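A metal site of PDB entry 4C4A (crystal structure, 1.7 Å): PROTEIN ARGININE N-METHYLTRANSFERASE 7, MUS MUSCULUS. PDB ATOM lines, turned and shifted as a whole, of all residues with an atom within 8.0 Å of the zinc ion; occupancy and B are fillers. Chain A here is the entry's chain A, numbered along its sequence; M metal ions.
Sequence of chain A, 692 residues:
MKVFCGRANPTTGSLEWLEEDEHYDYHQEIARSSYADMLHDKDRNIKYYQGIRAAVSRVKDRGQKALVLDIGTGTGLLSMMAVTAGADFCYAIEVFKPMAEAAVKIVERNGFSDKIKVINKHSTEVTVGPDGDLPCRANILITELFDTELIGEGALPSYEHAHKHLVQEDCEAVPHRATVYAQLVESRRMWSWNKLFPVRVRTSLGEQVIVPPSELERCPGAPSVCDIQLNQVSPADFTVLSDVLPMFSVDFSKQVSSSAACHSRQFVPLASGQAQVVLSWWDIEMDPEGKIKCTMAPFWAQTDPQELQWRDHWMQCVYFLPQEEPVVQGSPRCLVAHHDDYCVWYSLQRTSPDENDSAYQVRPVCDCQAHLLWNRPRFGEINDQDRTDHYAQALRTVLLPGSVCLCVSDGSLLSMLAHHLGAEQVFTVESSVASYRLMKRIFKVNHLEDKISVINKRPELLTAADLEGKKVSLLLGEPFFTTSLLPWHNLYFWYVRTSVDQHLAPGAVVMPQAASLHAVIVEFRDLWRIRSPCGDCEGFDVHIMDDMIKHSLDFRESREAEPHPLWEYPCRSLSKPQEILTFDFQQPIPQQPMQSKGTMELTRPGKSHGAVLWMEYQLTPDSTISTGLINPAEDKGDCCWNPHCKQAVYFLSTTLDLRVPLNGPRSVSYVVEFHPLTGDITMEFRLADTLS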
ATOM      1  N   ASN A 194      -5.684  21.018   1.722  1.00  0.00           N
ATOM      2  CA  ASN A 194      -6.300  21.885   0.703  1.00  0.00           C
ATOM      3  C   ASN A 194      -5.672  21.699  -0.691  1.00  0.00           C
ATOM      4  O   ASN A 194      -6.342  21.877  -1.721  1.00  0.00           O
ATOM      5  CB  ASN A 194      -6.166  23.354   1.134  1.00  0.00           C
ATOM      6  CG  ASN A 194      -6.725  24.343   0.107  1.00  0.00           C
ATOM      7  OD1 ASN A 194      -7.850  24.207  -0.367  1.00  0.00           O
ATOM      8  ND2 ASN A 194      -5.924  25.363  -0.235  1.00  0.00           N
ATOM      9  N   LYS A 195      -4.376  21.410  -0.736  1.00  0.00           N
ATOM     10  CA  LYS A 195      -3.692  21.234  -2.017  1.00  0.00           C
ATOM     11  C   LYS A 195      -3.156  19.822  -2.181  1.00  0.00           C
ATOM     12  O   LYS A 195      -2.691  19.224  -1.211  1.00  0.00           O
ATOM     13  CB  LYS A 195      -2.525  22.221  -2.177  1.00  0.00           C
ATOM     14  CG  LYS A 195      -2.898  23.696  -2.282  1.00  0.00           C
ATOM     15  CD  LYS A 195      -3.876  23.939  -3.434  1.00  0.00           C
ATOM     16  CE  LYS A 195      -4.132  25.423  -3.625  1.00  0.00           C
ATOM     17  NZ  LYS A 195      -5.198  25.650  -4.627  1.00  0.00           N
ATOM     18  N   GLU A 215      -5.452  23.289 -12.461  1.00  0.00           N
ATOM     19  CA  GLU A 215      -6.637  23.929 -11.896  1.00  0.00           C
ATOM     20  C   GLU A 215      -6.773  23.664 -10.392  1.00  0.00           C
ATOM     21  O   GLU A 215      -7.361  24.466  -9.680  1.00  0.00           O
ATOM     22  CB  GLU A 215      -7.908  23.485 -12.620  1.00  0.00           C
ATOM     23  CG  GLU A 215      -8.212  22.005 -12.518  1.00  0.00           C
ATOM     24  CD  GLU A 215      -7.668  21.203 -13.682  1.00  0.00           C
ATOM     25  OE1 GLU A 215      -6.687  21.630 -14.320  1.00  0.00           O
ATOM     26  OE2 GLU A 215      -8.244  20.132 -13.951  1.00  0.00           O
ATOM     27  N   LEU A 216      -6.229  22.538  -9.922  1.00  0.00           N
ATOM     28  CA  LEU A 216      -6.202  22.255  -8.478  1.00  0.00           C
ATOM     29  C   LEU A 216      -5.313  23.274  -7.782  1.00  0.00           C
ATOM     30  O   LEU A 216      -5.685  23.811  -6.743  1.00  0.00           O
ATOM     31  CB  LEU A 216      -5.704  20.840  -8.178  1.00  0.00           C
ATOM     32  CG  LEU A 216      -6.786  19.806  -7.861  1.00  0.00           C
ATOM     33  CD1 LEU A 216      -7.474  19.396  -9.161  1.00  0.00           C
ATOM     34  CD2 LEU A 216      -6.206  18.596  -7.130  1.00  0.00           C
ATOM     35  N   GLU A 217      -4.150  23.528  -8.385  1.00  0.00           N
ATOM     36  CA  GLU A 217      -3.182  24.503  -7.867  1.00  0.00           C
ATOM     37  C   GLU A 217      -3.785  25.896  -7.782  1.00  0.00           C
ATOM     38  O   GLU A 217      -3.404  26.678  -6.912  1.00  0.00           O
ATOM     39  CB  GLU A 217      -1.927  24.528  -8.745  1.00  0.00           C
ATOM     40  CG  GLU A 217      -1.344  23.146  -9.075  1.00  0.00           C
ATOM     41  CD  GLU A 217      -0.097  23.224  -9.963  1.00  0.00           C
ATOM     42  OE1 GLU A 217      -0.145  23.890 -11.033  1.00  0.00           O
ATOM     43  OE2 GLU A 217       0.926  22.609  -9.602  1.00  0.00           O
ATOM     44  N   ARG A 218      -4.716  26.210  -8.693  1.00  0.00           N
ATOM     45  CA  ARG A 218      -5.298  27.551  -8.770  1.00  0.00           C
ATOM     46  C   ARG A 218      -6.656  27.712  -8.074  1.00  0.00           C
ATOM     47  O   ARG A 218      -7.208  28.810  -8.031  1.00  0.00           O
ATOM     48  CB  ARG A 218      -5.452  27.976 -10.237  1.00  0.00           C
ATOM     49  CG  ARG A 218      -4.139  28.025 -11.023  1.00  0.00           C
ATOM     50  CD  ARG A 218      -4.391  28.529 -12.439  1.00  0.00           C
ATOM     51  NE  ARG A 218      -5.451  27.767 -13.107  1.00  0.00           N
ATOM     52  CZ  ARG A 218      -5.238  26.857 -14.044  1.00  0.00           C
ATOM     53  NH1 ARG A 218      -4.009  26.597 -14.465  1.00  0.00           N
ATOM     54  NH2 ARG A 218      -6.269  26.200 -14.588  1.00  0.00           N
ATOM     55  N   CYS A 219      -7.207  26.627  -7.541  1.00  0.00           N
ATOM     56  CA  CYS A 219      -8.540  26.645  -6.928  1.00  0.00           C
ATOM     57  C   CYS A 219      -8.570  27.283  -5.541  1.00  0.00           C
ATOM     58  O   CYS A 219      -7.671  27.092  -4.738  1.00  0.00           O
ATOM     59  CB  CYS A 219      -9.109  25.214  -6.836  1.00  0.00           C
ATOM     60  SG  CYS A 219     -10.836  25.104  -6.287  1.00  0.00           S
ATOM     61  N   PRO A 220      -9.627  28.055  -5.256  1.00  0.00           N
ATOM     62  CA  PRO A 220      -9.773  28.620  -3.909  1.00  0.00           C
ATOM     63  C   PRO A 220     -10.110  27.569  -2.843  1.00  0.00           C
ATOM     64  O   PRO A 220     -10.070  27.878  -1.645  1.00  0.00           O
ATOM     65  CB  PRO A 220     -10.932  29.601  -4.087  1.00  0.00           C
ATOM     66  CG  PRO A 220     -11.681  29.087  -5.281  1.00  0.00           C
ATOM     67  CD  PRO A 220     -10.629  28.570  -6.198  1.00  0.00           C
ATOM     68  N   GLY A 221     -10.421  26.351  -3.276  1.00  0.00           N
ATOM     69  CA  GLY A 221     -10.751  25.265  -2.365  1.00  0.00           C
ATOM     70  C   GLY A 221     -12.229  25.218  -2.037  1.00  0.00           C
ATOM     71  O   GLY A 221     -13.020  25.956  -2.614  1.00  0.00           O
ATOM     72  N   ALA A 222     -12.600  24.340  -1.111  1.00  0.00           N
ATOM     73  CA  ALA A 222     -13.990  24.228  -0.682  1.00  0.00           C
ATOM     74  C   ALA A 222     -14.376  25.420   0.171  1.00  0.00           C
ATOM     75  O   ALA A 222     -13.629  25.839   1.054  1.00  0.00           O
ATOM     76  CB  ALA A 222     -14.217  22.939   0.082  1.00  0.00           C
ATOM     77  N   PRO A 223     -15.556  25.985  -0.100  1.00  0.00           N
ATOM     78  CA  PRO A 223     -16.046  27.177   0.594  1.00  0.00           C
ATOM     79  C   PRO A 223     -16.699  26.810   1.917  1.00  0.00           C
ATOM     80  O   PRO A 223     -17.896  27.029   2.101  1.00  0.00           O
ATOM     81  CB  PRO A 223     -17.078  27.733  -0.375  1.00  0.00           C
ATOM     82  CG  PRO A 223     -17.611  26.525  -1.047  1.00  0.00           C
ATOM     83  CD  PRO A 223     -16.460  25.572  -1.179  1.00  0.00           C
ATOM     84  N   VAL A 365     -15.749  29.473  -5.318  1.00  0.00           N
ATOM     85  CA  VAL A 365     -16.198  28.097  -5.189  1.00  0.00           C
ATOM     86  C   VAL A 365     -15.159  27.182  -5.830  1.00  0.00           C
ATOM     87  O   VAL A 365     -14.279  27.657  -6.557  1.00  0.00           O
ATOM     88  CB  VAL A 365     -17.579  27.884  -5.844  1.00  0.00           C
ATOM     89  CG1 VAL A 365     -18.576  28.905  -5.293  1.00  0.00           C
ATOM     90  CG2 VAL A 365     -17.476  28.013  -7.349  1.00  0.00           C
ATOM     91  N   CYS A 366     -15.249  25.882  -5.540  1.00  0.00           N
ATOM     92  CA  CYS A 366     -14.313  24.928  -6.125  1.00  0.00           C
ATOM     93  C   CYS A 366     -14.571  24.772  -7.625  1.00  0.00           C
ATOM     94  O   CYS A 366     -15.671  24.435  -8.033  1.00  0.00           O
ATOM     95  CB  CYS A 366     -14.419  23.579  -5.427  1.00  0.00           C
ATOM     96  SG  CYS A 366     -13.465  22.284  -6.252  1.00  0.00           S
ATOM     97  N   ASP A 367     -13.561  25.037  -8.445  1.00  0.00           N
ATOM     98  CA  ASP A 367     -13.704  24.835  -9.891  1.00  0.00           C
ATOM     99  C   ASP A 367     -12.715  23.794 -10.411  1.00  0.00           C
ATOM    100  O   ASP A 367     -12.353  23.804 -11.579  1.00  0.00           O
ATOM    101  CB  ASP A 367     -13.529  26.161 -10.644  1.00  0.00           C
ATOM    102  CG  ASP A 367     -12.178  26.827 -10.413  1.00  0.00           C
ATOM    103  OD1 ASP A 367     -11.241  26.170  -9.929  1.00  0.00           O
ATOM    104  OD2 ASP A 367     -12.052  28.034 -10.719  1.00  0.00           O
ATOM    105  N   CYS A 368     -12.277  22.904  -9.534  1.00  0.00           N
ATOM    106  CA  CYS A 368     -11.294  21.883  -9.922  1.00  0.00           C
ATOM    107  C   CYS A 368     -11.811  20.472  -9.673  1.00  0.00           C
ATOM    108  O   CYS A 368     -11.122  19.501 -10.010  1.00  0.00           O
ATOM    109  CB  CYS A 368      -9.978  22.100  -9.174  1.00  0.00           C
ATOM    110  SG  CYS A 368      -9.962  21.476  -7.467  1.00  0.00           S
ATOM    111  N   GLN A 369     -13.023  20.375  -9.114  1.00  0.00           N
ATOM    112  CA  GLN A 369     -13.691  19.128  -8.700  1.00  0.00           C
ATOM    113  C   GLN A 369     -13.177  18.488  -7.404  1.00  0.00           C
ATOM    114  O   GLN A 369     -13.946  17.878  -6.656  1.00  0.00           O
ATOM    115  CB  GLN A 369     -13.619  18.062  -9.800  1.00  0.00           C
ATOM    116  CG  GLN A 369     -14.456  18.349 -11.027  1.00  0.00           C
ATOM    117  CD  GLN A 369     -14.766  17.066 -11.766  1.00  0.00           C
ATOM    118  OE1 GLN A 369     -15.780  16.415 -11.513  1.00  0.00           O
ATOM    119  NE2 GLN A 369     -13.879  16.672 -12.668  1.00  0.00           N
ATOM    120  N   ALA A 370     -11.881  18.602  -7.141  1.00  0.00           N
ATOM    121  CA  ALA A 370     -11.248  17.831  -6.059  1.00  0.00           C
ATOM    122  C   ALA A 370     -11.803  18.153  -4.675  1.00  0.00           C
ATOM    123  O   ALA A 370     -11.932  17.263  -3.832  1.00  0.00           O
ATOM    124  CB  ALA A 370      -9.731  18.057  -6.074  1.00  0.00           C
ATOM    125  N   HIS A 371     -12.132  19.419  -4.427  1.00  0.00           N
ATOM    126  CA  HIS A 371     -12.522  19.812  -3.069  1.00  0.00           C
ATOM    127  C   HIS A 371     -13.978  19.438  -2.768  1.00  0.00           C
ATOM    128  O   HIS A 371     -14.412  19.508  -1.618  1.00  0.00           O
ATOM    129  CB  HIS A 371     -12.277  21.309  -2.856  1.00  0.00           C
ATOM    130  CG  HIS A 371     -10.847  21.689  -3.032  1.00  0.00           C
ATOM    131  ND1 HIS A 371     -10.337  22.159  -4.232  1.00  0.00           N
ATOM    132  CD2 HIS A 371      -9.791  21.605  -2.194  1.00  0.00           C
ATOM    133  CE1 HIS A 371      -9.043  22.380  -4.110  1.00  0.00           C
ATOM    134  NE2 HIS A 371      -8.686  22.052  -2.875  1.00  0.00           N
ATOM    135  N   LEU A 372     -14.715  19.046  -3.798  1.00  0.00           N
ATOM    136  CA  LEU A 372     -16.060  18.530  -3.626  1.00  0.00           C
ATOM    137  C   LEU A 372     -16.056  17.016  -3.409  1.00  0.00           C
ATOM    138  O   LEU A 372     -17.064  16.451  -2.974  1.00  0.00           O
ATOM    139  CB  LEU A 372     -16.930  18.867  -4.836  1.00  0.00           C
ATOM    140  CG  LEU A 372     -17.115  20.344  -5.186  1.00  0.00           C
ATOM    141  CD1 LEU A 372     -17.928  20.479  -6.466  1.00  0.00           C
ATOM    142  CD2 LEU A 372     -17.768  21.093  -4.052  1.00  0.00           C
ATOM    143  N   LEU A 373     -14.934  16.362  -3.715  1.00  0.00           N
ATOM    144  CA  LEU A 373     -14.848  14.901  -3.671  1.00  0.00           C
ATOM    145  C   LEU A 373     -13.966  14.347  -2.563  1.00  0.00           C
ATOM    146  O   LEU A 373     -14.227  13.255  -2.042  1.00  0.00           O
ATOM    147  CB  LEU A 373     -14.331  14.388  -5.011  1.00  0.00           C
ATOM    148  CG  LEU A 373     -15.231  14.694  -6.207  1.00  0.00           C
ATOM    149  CD1 LEU A 373     -14.546  14.299  -7.504  1.00  0.00           C
ATOM    150  CD2 LEU A 373     -16.588  13.990  -6.063  1.00  0.00           C
ATOM    151  N   PHE A 379      -7.436  14.608   1.764  1.00  0.00           N
ATOM    152  CA  PHE A 379      -6.329  15.361   1.184  1.00  0.00           C
ATOM    153  C   PHE A 379      -5.029  15.102   1.954  1.00  0.00           C
ATOM    154  O   PHE A 379      -3.988  14.825   1.353  1.00  0.00           O
ATOM    155  CB  PHE A 379      -6.635  16.873   1.180  1.00  0.00           C
ATOM    156  CG  PHE A 379      -7.159  17.398  -0.131  1.00  0.00           C
ATOM    157  CD1 PHE A 379      -6.284  17.771  -1.148  1.00  0.00           C
ATOM    158  CD2 PHE A 379      -8.526  17.557  -0.329  1.00  0.00           C
ATOM    159  CE1 PHE A 379      -6.771  18.291  -2.356  1.00  0.00           C
ATOM    160  CE2 PHE A 379      -9.017  18.072  -1.515  1.00  0.00           C
ATOM    161  CZ  PHE A 379      -8.128  18.429  -2.539  1.00  0.00           C
HETATM  162 ZN    ZN M   1     -11.227  22.830  -6.067  1.00  0.00          ZN
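SG of Cys 219 sits close to N of Asp 367, at 3.5 Å.
O of Asn 194 sits at hydrogen-bond distance from NE2 of His 371 (2.6 Å).
The side-chain sulfur of Cys 366 lies close to the backbone NH of Gln 369.
The backbone NH (N) of Ala 370 lies close to the side-chain sulfur (SG) of Cys 368 (3.5 Å).
N of Gly 221 sits close to SG of Cys 219 (3.3 Å).
The backbone carbonyl oxygen (O) of Cys 219 lies within hydrogen-bond range of the side-chain amino group (NZ) of Lys 195 (2.9 Å).
Merely in contact with the zinc ion: Asp 367 (3.997 Å).
Five residues have an atom within 4 Å of the zinc ion: Cys 219, Cys 366, Asp 367, Cys 368 and His 371.
The nearest printed residue that does not touch the zinc ion is Gln 369 (4.3 Å).
The zinc ion is bound by ND1 of His 371 (2.1 Å), SG of Cys 366 (2.3 Å), SG of Cys 219 (2.3 Å) and SG of Cys 368 (2.3 Å).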
